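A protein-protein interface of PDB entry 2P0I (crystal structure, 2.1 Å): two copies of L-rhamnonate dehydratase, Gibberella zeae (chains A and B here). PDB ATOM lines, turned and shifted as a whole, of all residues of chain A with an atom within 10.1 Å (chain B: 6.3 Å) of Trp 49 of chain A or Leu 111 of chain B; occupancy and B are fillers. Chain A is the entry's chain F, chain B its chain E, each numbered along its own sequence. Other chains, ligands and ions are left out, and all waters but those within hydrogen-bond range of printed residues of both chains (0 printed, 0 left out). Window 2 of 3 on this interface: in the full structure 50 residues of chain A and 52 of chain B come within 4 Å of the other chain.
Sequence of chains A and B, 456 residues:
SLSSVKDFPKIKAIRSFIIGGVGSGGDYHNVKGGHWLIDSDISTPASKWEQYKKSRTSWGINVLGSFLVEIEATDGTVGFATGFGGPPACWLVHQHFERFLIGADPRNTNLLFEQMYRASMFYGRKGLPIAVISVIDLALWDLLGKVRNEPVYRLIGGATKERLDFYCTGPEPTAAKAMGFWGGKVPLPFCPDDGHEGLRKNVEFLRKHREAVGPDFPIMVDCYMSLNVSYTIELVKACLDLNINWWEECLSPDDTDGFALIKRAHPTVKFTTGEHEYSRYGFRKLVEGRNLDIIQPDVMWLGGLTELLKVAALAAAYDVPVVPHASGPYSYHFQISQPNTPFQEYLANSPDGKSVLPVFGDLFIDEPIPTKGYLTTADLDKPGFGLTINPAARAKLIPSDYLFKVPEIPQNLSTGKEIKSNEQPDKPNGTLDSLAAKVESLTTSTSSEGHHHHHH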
ATOM      1  N   ILE A  42      -2.655  -5.838   6.958  1.00  0.00           N
ATOM      2  CA  ILE A  42      -4.004  -6.385   6.742  1.00  0.00           C
ATOM      3  C   ILE A  42      -4.111  -6.841   5.280  1.00  0.00           C
ATOM      4  O   ILE A  42      -3.768  -6.084   4.363  1.00  0.00           O
ATOM      5  CB  ILE A  42      -5.125  -5.328   7.065  1.00  0.00           C
ATOM      6  CG1 ILE A  42      -5.210  -5.047   8.573  1.00  0.00           C
ATOM      7  CG2 ILE A  42      -6.500  -5.785   6.552  1.00  0.00           C
ATOM      8  CD1 ILE A  42      -5.914  -3.739   8.932  1.00  0.00           C
ATOM      9  N   THR A  44      -5.757  -7.458   1.903  1.00  0.00           N
ATOM     10  CA  THR A  44      -6.821  -6.785   1.141  1.00  0.00           C
ATOM     11  C   THR A  44      -6.800  -7.303  -0.311  1.00  0.00           C
ATOM     12  O   THR A  44      -5.807  -7.916  -0.718  1.00  0.00           O
ATOM     13  CB  THR A  44      -6.630  -5.235   1.145  1.00  0.00           C
ATOM     14  OG1 THR A  44      -5.377  -4.893   0.540  1.00  0.00           O
ATOM     15  CG2 THR A  44      -6.690  -4.674   2.563  1.00  0.00           C
ATOM     16  N   PRO A  45      -7.892  -7.083  -1.091  1.00  0.00           N
ATOM     17  CA  PRO A  45      -7.867  -7.389  -2.533  1.00  0.00           C
ATOM     18  C   PRO A  45      -6.763  -6.707  -3.356  1.00  0.00           C
ATOM     19  O   PRO A  45      -6.381  -7.219  -4.415  1.00  0.00           O
ATOM     20  CB  PRO A  45      -9.247  -6.922  -3.016  1.00  0.00           C
ATOM     21  CG  PRO A  45     -10.114  -7.001  -1.805  1.00  0.00           C
ATOM     22  CD  PRO A  45      -9.223  -6.593  -0.674  1.00  0.00           C
ATOM     23  N   ALA A  46      -6.258  -5.574  -2.870  1.00  0.00           N
ATOM     24  CA  ALA A  46      -5.203  -4.833  -3.563  1.00  0.00           C
ATOM     25  C   ALA A  46      -3.779  -5.136  -3.061  1.00  0.00           C
ATOM     26  O   ALA A  46      -2.815  -4.483  -3.480  1.00  0.00           O
ATOM     27  CB  ALA A  46      -5.493  -3.332  -3.512  1.00  0.00           C
ATOM     28  N   SER A  47      -3.641  -6.138  -2.189  1.00  0.00           N
ATOM     29  CA  SER A  47      -2.327  -6.540  -1.658  1.00  0.00           C
ATOM     30  C   SER A  47      -1.492  -7.343  -2.663  1.00  0.00           C
ATOM     31  O   SER A  47      -0.332  -7.685  -2.385  1.00  0.00           O
ATOM     32  CB  SER A  47      -2.470  -7.316  -0.343  1.00  0.00           C
ATOM     33  OG  SER A  47      -3.159  -6.570   0.645  1.00  0.00           O
ATOM     34  N   LYS A  48      -2.097  -7.630  -3.820  1.00  0.00           N
ATOM     35  CA  LYS A  48      -1.426  -8.160  -5.014  1.00  0.00           C
ATOM     36  C   LYS A  48      -0.222  -7.326  -5.458  1.00  0.00           C
ATOM     37  O   LYS A  48       0.794  -7.873  -5.899  1.00  0.00           O
ATOM     38  CB  LYS A  48      -2.418  -8.249  -6.184  1.00  0.00           C
ATOM     39  CG  LYS A  48      -3.638  -9.140  -5.948  1.00  0.00           C
ATOM     40  CD  LYS A  48      -4.502  -9.271  -7.206  1.00  0.00           C
ATOM     41  CE  LYS A  48      -3.806 -10.060  -8.323  1.00  0.00           C
ATOM     42  NZ  LYS A  48      -3.940 -11.539  -8.187  1.00  0.00           N
ATOM     43  N   TRP A  49      -0.348  -6.004  -5.342  1.00  0.00           N
ATOM     44  CA  TRP A  49       0.642  -5.078  -5.881  1.00  0.00           C
ATOM     45  C   TRP A  49       1.354  -4.322  -4.770  1.00  0.00           C
ATOM     46  O   TRP A  49       0.736  -3.957  -3.762  1.00  0.00           O
ATOM     47  CB  TRP A  49      -0.009  -4.129  -6.892  1.00  0.00           C
ATOM     48  CG  TRP A  49      -0.882  -4.874  -7.853  1.00  0.00           C
ATOM     49  CD1 TRP A  49      -0.472  -5.621  -8.923  1.00  0.00           C
ATOM     50  CD2 TRP A  49      -2.310  -4.989  -7.808  1.00  0.00           C
ATOM     51  NE1 TRP A  49      -1.555  -6.183  -9.553  1.00  0.00           N
ATOM     52  CE2 TRP A  49      -2.697  -5.809  -8.896  1.00  0.00           C
ATOM     53  CE3 TRP A  49      -3.303  -4.473  -6.962  1.00  0.00           C
ATOM     54  CZ2 TRP A  49      -4.031  -6.126  -9.161  1.00  0.00           C
ATOM     55  CZ3 TRP A  49      -4.633  -4.786  -7.227  1.00  0.00           C
ATOM     56  CH2 TRP A  49      -4.984  -5.609  -8.317  1.00  0.00           C
ATOM     57  N   GLU A  50       2.653  -4.096  -4.973  1.00  0.00           N
ATOM     58  CA  GLU A  50       3.608  -3.799  -3.899  1.00  0.00           C
ATOM     59  C   GLU A  50       3.341  -2.467  -3.193  1.00  0.00           C
ATOM     60  O   GLU A  50       3.515  -2.354  -1.976  1.00  0.00           O
ATOM     61  CB  GLU A  50       5.046  -3.847  -4.438  1.00  0.00           C
ATOM     62  CG  GLU A  50       6.151  -3.912  -3.370  1.00  0.00           C
ATOM     63  CD  GLU A  50       5.969  -5.058  -2.379  1.00  0.00           C
ATOM     64  OE1 GLU A  50       5.882  -6.228  -2.815  1.00  0.00           O
ATOM     65  OE2 GLU A  50       5.918  -4.787  -1.161  1.00  0.00           O
ATOM     66  N   GLN A  51       2.894  -1.478  -3.963  1.00  0.00           N
ATOM     67  CA  GLN A  51       2.689  -0.122  -3.461  1.00  0.00           C
ATOM     68  C   GLN A  51       1.304   0.072  -2.825  1.00  0.00           C
ATOM     69  O   GLN A  51       0.980   1.161  -2.336  1.00  0.00           O
ATOM     70  CB  GLN A  51       2.966   0.909  -4.569  1.00  0.00           C
ATOM     71  CG  GLN A  51       1.838   1.098  -5.582  1.00  0.00           C
ATOM     72  CD  GLN A  51       2.085   0.432  -6.934  1.00  0.00           C
ATOM     73  OE1 GLN A  51       1.662   0.953  -7.967  1.00  0.00           O
ATOM     74  NE2 GLN A  51       2.750  -0.720  -6.933  1.00  0.00           N
ATOM     75  N   TYR A  52       0.503  -0.994  -2.821  1.00  0.00           N
ATOM     76  CA  TYR A  52      -0.839  -0.956  -2.242  1.00  0.00           C
ATOM     77  C   TYR A  52      -1.054  -1.941  -1.094  1.00  0.00           C
ATOM     78  O   TYR A  52      -2.190  -2.162  -0.667  1.00  0.00           O
ATOM     79  CB  TYR A  52      -1.913  -1.125  -3.328  1.00  0.00           C
ATOM     80  CG  TYR A  52      -1.844  -0.069  -4.410  1.00  0.00           C
ATOM     81  CD1 TYR A  52      -2.058   1.279  -4.112  1.00  0.00           C
ATOM     82  CD2 TYR A  52      -1.547  -0.415  -5.729  1.00  0.00           C
ATOM     83  CE1 TYR A  52      -1.984   2.253  -5.099  1.00  0.00           C
ATOM     84  CE2 TYR A  52      -1.476   0.552  -6.726  1.00  0.00           C
ATOM     85  CZ  TYR A  52      -1.691   1.885  -6.402  1.00  0.00           C
ATOM     86  OH  TYR A  52      -1.619   2.852  -7.379  1.00  0.00           O
ATOM     87  N   LYS A  53       0.033  -2.518  -0.584  1.00  0.00           N
ATOM     88  CA  LYS A  53      -0.069  -3.536   0.460  1.00  0.00           C
ATOM     89  C   LYS A  53       0.315  -3.085   1.873  1.00  0.00           C
ATOM     90  O   LYS A  53      -0.216  -3.608   2.855  1.00  0.00           O
ATOM     91  CB  LYS A  53       0.631  -4.843   0.055  1.00  0.00           C
ATOM     92  CG  LYS A  53       2.156  -4.808   0.006  1.00  0.00           C
ATOM     93  CD  LYS A  53       2.713  -5.889  -0.922  1.00  0.00           C
ATOM     94  CE  LYS A  53       2.505  -7.301  -0.383  1.00  0.00           C
ATOM     95  NZ  LYS A  53       3.543  -7.689   0.610  1.00  0.00           N
ATOM     96  N   LYS A  54       1.222  -2.112   1.970  1.00  0.00           N
ATOM     97  CA  LYS A  54       1.621  -1.535   3.256  1.00  0.00           C
ATOM     98  C   LYS A  54       0.536  -0.629   3.833  1.00  0.00           C
ATOM     99  O   LYS A  54       0.292  -0.630   5.040  1.00  0.00           O
ATOM    100  CB  LYS A  54       2.938  -0.765   3.117  1.00  0.00           C
ATOM    101  CG  LYS A  54       4.159  -1.507   3.647  1.00  0.00           C
ATOM    102  CD  LYS A  54       4.535  -1.030   5.048  1.00  0.00           C
ATOM    103  CE  LYS A  54       5.223  -2.128   5.854  1.00  0.00           C
ATOM    104  NZ  LYS A  54       6.692  -2.179   5.621  1.00  0.00           N
ATOM    105  N   SER A  55      -0.113   0.131   2.956  1.00  0.00           N
ATOM    106  CA  SER A  55      -1.085   1.144   3.357  1.00  0.00           C
ATOM    107  C   SER A  55      -2.466   0.828   2.774  1.00  0.00           C
ATOM    108  O   SER A  55      -2.610   0.626   1.565  1.00  0.00           O
ATOM    109  CB  SER A  55      -0.601   2.533   2.913  1.00  0.00           C
ATOM    110  OG  SER A  55      -1.522   3.553   3.256  1.00  0.00           O
ATOM    111  N   ARG A  56      -3.471   0.779   3.646  1.00  0.00           N
ATOM    112  CA  ARG A  56      -4.857   0.535   3.239  1.00  0.00           C
ATOM    113  C   ARG A  56      -5.481   1.762   2.570  1.00  0.00           C
ATOM    114  O   ARG A  56      -6.361   1.632   1.712  1.00  0.00           O
ATOM    115  CB  ARG A  56      -5.697   0.100   4.443  1.00  0.00           C
ATOM    116  CG  ARG A  56      -6.672  -1.032   4.154  1.00  0.00           C
ATOM    117  CD  ARG A  56      -6.587  -2.120   5.219  1.00  0.00           C
ATOM    118  NE  ARG A  56      -7.463  -1.867   6.363  1.00  0.00           N
ATOM    119  CZ  ARG A  56      -8.647  -2.446   6.562  1.00  0.00           C
ATOM    120  NH1 ARG A  56      -9.356  -2.139   7.640  1.00  0.00           N
ATOM    121  NH2 ARG A  56      -9.128  -3.330   5.693  1.00  0.00           N
ATOM    122  N   SER A  58      -3.813   3.717   0.601  1.00  0.00           N
ATOM    123  CA  SER A  58      -3.107   3.924  -0.664  1.00  0.00           C
ATOM    124  C   SER A  58      -3.889   3.456  -1.898  1.00  0.00           C
ATOM    125  O   SER A  58      -3.749   4.038  -2.976  1.00  0.00           O
ATOM    126  CB  SER A  58      -1.710   3.291  -0.623  1.00  0.00           C
ATOM    127  OG  SER A  58      -1.776   1.881  -0.718  1.00  0.00           O
ATOM    128  N   TRP A  59      -4.712   2.417  -1.733  1.00  0.00           N
ATOM    129  CA  TRP A  59      -5.674   2.020  -2.771  1.00  0.00           C
ATOM    130  C   TRP A  59      -7.067   2.635  -2.600  1.00  0.00           C
ATOM    131  O   TRP A  59      -7.924   2.495  -3.476  1.00  0.00           O
ATOM    132  CB  TRP A  59      -5.754   0.494  -2.921  1.00  0.00           C
ATOM    133  CG  TRP A  59      -6.078  -0.242  -1.662  1.00  0.00           C
ATOM    134  CD1 TRP A  59      -5.187  -0.730  -0.743  1.00  0.00           C
ATOM    135  CD2 TRP A  59      -7.381  -0.596  -1.182  1.00  0.00           C
ATOM    136  NE1 TRP A  59      -5.856  -1.359   0.284  1.00  0.00           N
ATOM    137  CE2 TRP A  59      -7.204  -1.289   0.041  1.00  0.00           C
ATOM    138  CE3 TRP A  59      -8.683  -0.390  -1.659  1.00  0.00           C
ATOM    139  CZ2 TRP A  59      -8.280  -1.779   0.788  1.00  0.00           C
ATOM    140  CZ3 TRP A  59      -9.751  -0.874  -0.917  1.00  0.00           C
ATOM    141  CH2 TRP A  59      -9.542  -1.565   0.292  1.00  0.00           C
ATOM    142  N   CYS A 191      -1.428 -11.762   2.116  1.00  0.00           N
ATOM    143  CA  CYS A 191      -2.289 -12.171   1.005  1.00  0.00           C
ATOM    144  C   CYS A 191      -1.687 -13.392   0.280  1.00  0.00           C
ATOM    145  O   CYS A 191      -0.523 -13.716   0.512  1.00  0.00           O
ATOM    146  CB  CYS A 191      -2.501 -10.979   0.056  1.00  0.00           C
ATOM    147  SG  CYS A 191      -1.158 -10.687  -1.121  1.00  0.00           S
ATOM    148  N   PRO A 192      -2.472 -14.077  -0.593  1.00  0.00           N
ATOM    149  CA  PRO A 192      -1.953 -15.207  -1.385  1.00  0.00           C
ATOM    150  C   PRO A 192      -0.676 -14.942  -2.194  1.00  0.00           C
ATOM    151  O   PRO A 192       0.111 -15.867  -2.412  1.00  0.00           O
ATOM    152  CB  PRO A 192      -3.112 -15.529  -2.335  1.00  0.00           C
ATOM    153  CG  PRO A 192      -4.317 -15.102  -1.592  1.00  0.00           C
ATOM    154  CD  PRO A 192      -3.906 -13.857  -0.869  1.00  0.00           C
ATOM    155  N   ASP A 193      -0.467 -13.696  -2.616  1.00  0.00           N
ATOM    156  CA  ASP A 193       0.650 -13.359  -3.493  1.00  0.00           C
ATOM    157  C   ASP A 193       1.970 -13.161  -2.751  1.00  0.00           C
ATOM    158  O   ASP A 193       3.029 -13.022  -3.372  1.00  0.00           O
ATOM    159  CB  ASP A 193       0.304 -12.160  -4.373  1.00  0.00           C
ATOM    160  CG  ASP A 193      -0.701 -12.512  -5.452  1.00  0.00           C
ATOM    161  OD1 ASP A 193      -0.478 -13.502  -6.184  1.00  0.00           O
ATOM    162  OD2 ASP A 193      -1.722 -11.806  -5.568  1.00  0.00           O
ATOM    163  N   ASP A 194       1.901 -13.184  -1.422  1.00  0.00           N
ATOM    164  CA  ASP A 194       3.070 -13.385  -0.578  1.00  0.00           C
ATOM    165  C   ASP A 194       3.485 -14.859  -0.456  1.00  0.00           C
ATOM    166  O   ASP A 194       4.423 -15.182   0.280  1.00  0.00           O
ATOM    167  CB  ASP A 194       2.843 -12.747   0.802  1.00  0.00           C
ATOM    168  CG  ASP A 194       2.629 -11.235   0.720  1.00  0.00           C
ATOM    169  OD1 ASP A 194       3.381 -10.572  -0.025  1.00  0.00           O
ATOM    170  OD2 ASP A 194       1.707 -10.706   1.387  1.00  0.00           O
ATOM    171  N   ASN B 108      -0.494  -1.372 -20.367  1.00  0.00           N
ATOM    172  CA  ASN B 108      -0.831  -2.195 -19.207  1.00  0.00           C
ATOM    173  C   ASN B 108      -2.326  -2.268 -18.897  1.00  0.00           C
ATOM    174  O   ASN B 108      -2.719  -2.113 -17.747  1.00  0.00           O
ATOM    175  CB  ASN B 108      -0.086  -1.702 -17.960  1.00  0.00           C
ATOM    176  CG  ASN B 108       1.384  -2.093 -17.950  1.00  0.00           C
ATOM    177  OD1 ASN B 108       1.855  -2.832 -18.808  1.00  0.00           O
ATOM    178  ND2 ASN B 108       2.116  -1.590 -16.965  1.00  0.00           N
ATOM    179  N   THR B 109      -3.148  -2.536 -19.912  1.00  0.00           N
ATOM    180  CA  THR B 109      -4.611  -2.600 -19.762  1.00  0.00           C
ATOM    181  C   THR B 109      -5.078  -3.652 -18.741  1.00  0.00           C
ATOM    182  O   THR B 109      -6.016  -3.418 -17.977  1.00  0.00           O
ATOM    183  CB  THR B 109      -5.291  -2.907 -21.104  1.00  0.00           C
ATOM    184  OG1 THR B 109      -4.620  -4.004 -21.738  1.00  0.00           O
ATOM    185  CG2 THR B 109      -5.245  -1.700 -22.023  1.00  0.00           C
ATOM    186  N   ASN B 110      -4.414  -4.805 -18.738  1.00  0.00           N
ATOM    187  CA  ASN B 110      -4.701  -5.868 -17.788  1.00  0.00           C
ATOM    188  C   ASN B 110      -4.434  -5.483 -16.341  1.00  0.00           C
ATOM    189  O   ASN B 110      -5.249  -5.796 -15.467  1.00  0.00           O
ATOM    190  CB  ASN B 110      -3.931  -7.148 -18.144  1.00  0.00           C
ATOM    191  CG  ASN B 110      -4.627  -7.984 -19.205  1.00  0.00           C
ATOM    192  OD1 ASN B 110      -5.795  -7.757 -19.534  1.00  0.00           O
ATOM    193  ND2 ASN B 110      -3.904  -8.963 -19.748  1.00  0.00           N
ATOM    194  N   LEU B 111      -3.309  -4.807 -16.088  1.00  0.00           N
ATOM    195  CA  LEU B 111      -2.983  -4.321 -14.731  1.00  0.00           C
ATOM    196  C   LEU B 111      -4.018  -3.320 -14.231  1.00  0.00           C
ATOM    197  O   LEU B 111      -4.560  -3.445 -13.117  1.00  0.00           O
ATOM    198  CB  LEU B 111      -1.592  -3.671 -14.686  1.00  0.00           C
ATOM    199  CG  LEU B 111      -1.123  -3.195 -13.305  1.00  0.00           C
ATOM    200  CD1 LEU B 111      -1.055  -4.341 -12.327  1.00  0.00           C
ATOM    201  CD2 LEU B 111       0.222  -2.500 -13.375  1.00  0.00           C
ATOM    202  N   LEU B 112      -4.293  -2.337 -15.082  1.00  0.00           N
ATOM    203  CA  LEU B 112      -5.063  -1.175 -14.698  1.00  0.00           C
ATOM    204  C   LEU B 112      -6.510  -1.534 -14.397  1.00  0.00           C
ATOM    205  O   LEU B 112      -7.107  -0.958 -13.485  1.00  0.00           O
ATOM    206  CB  LEU B 112      -4.929  -0.061 -15.742  1.00  0.00           C
ATOM    207  CG  LEU B 112      -3.510   0.536 -15.803  1.00  0.00           C
ATOM    208  CD1 LEU B 112      -3.278   1.373 -17.033  1.00  0.00           C
ATOM    209  CD2 LEU B 112      -3.222   1.335 -14.560  1.00  0.00           C
ATOM    210  N   PHE B 113      -7.055  -2.519 -15.110  1.00  0.00           N
ATOM    211  CA  PHE B 113      -8.408  -2.963 -14.811  1.00  0.00           C
ATOM    212  C   PHE B 113      -8.526  -3.639 -13.445  1.00  0.00           C
ATOM    213  O   PHE B 113      -9.431  -3.309 -12.670  1.00  0.00           O
ATOM    214  CB  PHE B 113      -8.993  -3.874 -15.890  1.00  0.00           C
ATOM    215  CG  PHE B 113     -10.352  -4.398 -15.531  1.00  0.00           C
ATOM    216  CD1 PHE B 113     -11.488  -3.667 -15.844  1.00  0.00           C
ATOM    217  CD2 PHE B 113     -10.493  -5.590 -14.816  1.00  0.00           C
ATOM    218  CE1 PHE B 113     -12.745  -4.127 -15.486  1.00  0.00           C
ATOM    219  CE2 PHE B 113     -11.745  -6.056 -14.449  1.00  0.00           C
ATOM    220  CZ  PHE B 113     -12.877  -5.323 -14.791  1.00  0.00           C
ATOM    221  N   GLU B 114      -7.630  -4.593 -13.179  1.00  0.00           N
ATOM    222  CA  GLU B 114      -7.641  -5.379 -11.943  1.00  0.00           C
ATOM    223  C   GLU B 114      -7.438  -4.480 -10.740  1.00  0.00           C
ATOM    224  O   GLU B 114      -8.102  -4.653  -9.723  1.00  0.00           O
ATOM    225  CB  GLU B 114      -6.534  -6.443 -11.946  1.00  0.00           C
ATOM    226  CG  GLU B 114      -6.668  -7.563 -12.976  1.00  0.00           C
ATOM    227  CD  GLU B 114      -8.019  -8.260 -12.963  1.00  0.00           C
ATOM    228  OE1 GLU B 114      -8.445  -8.745 -11.889  1.00  0.00           O
ATOM    229  OE2 GLU B 114      -8.647  -8.329 -14.044  1.00  0.00           O
ATOM    230  N   GLN B 115      -6.515  -3.526 -10.871  1.00  0.00           N
ATOM    231  CA  GLN B 115      -6.259  -2.530  -9.833  1.00  0.00           C
ATOM    232  C   GLN B 115      -7.497  -1.711  -9.503  1.00  0.00           C
ATOM    233  O   GLN B 115      -7.931  -1.678  -8.353  1.00  0.00           O
ATOM    234  CB  GLN B 115      -5.103  -1.619 -10.233  1.00  0.00           C
ATOM    235  CG  GLN B 115      -3.752  -2.198  -9.861  1.00  0.00           C
ATOM    236  CD  GLN B 115      -2.592  -1.325 -10.288  1.00  0.00           C
ATOM    237  OE1 GLN B 115      -2.721  -0.476 -11.173  1.00  0.00           O
ATOM    238  NE2 GLN B 115      -1.444  -1.539  -9.665  1.00  0.00           N
ATOM    239  N   MET B 116      -8.079  -1.087 -10.524  1.00  0.00           N
ATOM    240  CA  MET B 116      -9.306  -0.330 -10.369  1.00  0.00           C
ATOM    241  C   MET B 116     -10.457  -1.163  -9.801  1.00  0.00           C
ATOM    242  O   MET B 116     -11.169  -0.697  -8.918  1.00  0.00           O
ATOM    243  CB  MET B 116      -9.696   0.325 -11.691  1.00  0.00           C
ATOM    244  CG  MET B 116      -8.840   1.532 -12.050  1.00  0.00           C
ATOM    245  SD  MET B 116      -9.295   2.366 -13.768  1.00  0.00           S
ATOM    246  CE  MET B 116     -11.107   2.842 -13.465  1.00  0.00           C
ATOM    247  N   ARG B 118     -10.447  -4.220  -8.079  1.00  0.00           N
ATOM    248  CA  ARG B 118     -10.238  -4.817  -6.768  1.00  0.00           C
ATOM    249  C   ARG B 118     -10.117  -3.754  -5.678  1.00  0.00           C
ATOM    250  O   ARG B 118     -10.492  -4.000  -4.526  1.00  0.00           O
ATOM    251  CB  ARG B 118      -9.041  -5.785  -6.782  1.00  0.00           C
ATOM    252  CG  ARG B 118      -9.278  -7.023  -7.666  1.00  0.00           C
ATOM    253  CD  ARG B 118      -8.115  -8.004  -7.672  1.00  0.00           C
ATOM    254  NE  ARG B 118      -7.811  -8.572  -6.354  1.00  0.00           N
ATOM    255  CZ  ARG B 118      -8.445  -9.603  -5.798  1.00  0.00           C
ATOM    256  NH1 ARG B 118      -9.447 -10.204  -6.426  1.00  0.00           N
ATOM    257  NH2 ARG B 118      -8.067 -10.045  -4.607  1.00  0.00           N
ATOM    258  N   ALA B 119      -9.628  -2.569  -6.055  1.00  0.00           N
ATOM    259  CA  ALA B 119      -9.600  -1.422  -5.147  1.00  0.00           C
ATOM    260  C   ALA B 119     -10.975  -0.807  -4.907  1.00  0.00           C
ATOM    261  O   ALA B 119     -11.215  -0.239  -3.838  1.00  0.00           O
ATOM    262  CB  ALA B 119      -8.630  -0.373  -5.628  1.00  0.00           C
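Of the 20 printed residues of chain A, 5 touch a printed residue of chain B. Along chain A the printed residues that touch a printed residue of chain B span positions 45 to 59. Hydrophobic or aromatic side chains of chain B that line the printed part of chain A: Leu 111 and Ala 119. Among the printed residues, 8 pairs touch across the chains.
No position is printed for both chains.
O of Pro 45 of chain A lies within hydrogen-bond range of NE of Arg 118 of chain B.
The side-chain carboxylate of Asp 193 of chain A is in salt-bridge range of the side-chain amino group of Lys 48 of chain A (3.4 Å). The indole nitrogen of Trp 59 of chain A sits at hydrogen-bond distance from the backbone carbonyl oxygen of Arg 56 of chain A, 3.4 Å away.
CD of Lys 48 of chain A touches NE of Arg 118 of chain B, 3.5 Å away. Leu 111 of chain B touches Trp 49 of chain A (CD1 to NE1, 3.4 Å). Trp 49 of chain A touches Glu 114 of chain B (CH2 to O, 3.6 Å). Gln 115 of chain B touches Trp 49 of chain A (N to CH2, 3.6 Å). CH2 of Trp 49 of chain A touches CD of Arg 118 of chain B (3.99 Å). Gln 115 of chain B touches Tyr 52 of chain A (NE2 to CE2, 3.6 Å). Ala 119 of chain B touches Trp 59 of chain A.
Of the printed residues of chain B, Trp 49 of chain A touches Leu 111 (3.4 Å), Glu 114 (3.6 Å), Gln 115 (3.6 Å) and Arg 118 (3.99 Å). Leu 111 of chain B touches one residue of chain A. No residue of chain A comes within 4 Å of Asn 110 of chain B. Of chain A, only Trp 49 and Tyr 52 come within 4 Å of Gln 115 of chain B. Of the printed residues of chain B, Trp 59 of chain A touches Ala 119. Of the printed residues of chain A, Arg 118 of chain B touches Pro 45, Lys 48 and Trp 49. The nearest printed residue of chain B that does not touch Trp 49 of chain A is Ala 119 of chain B (5.6 Å). The nearest residue of chain A that does not touch Leu 111 of chain B is Gln 51 of chain A (6.6 Å). The nearest printed residue of chain A that does not touch Arg 118 of chain B is Ala 46 of chain A (4.8 Å).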
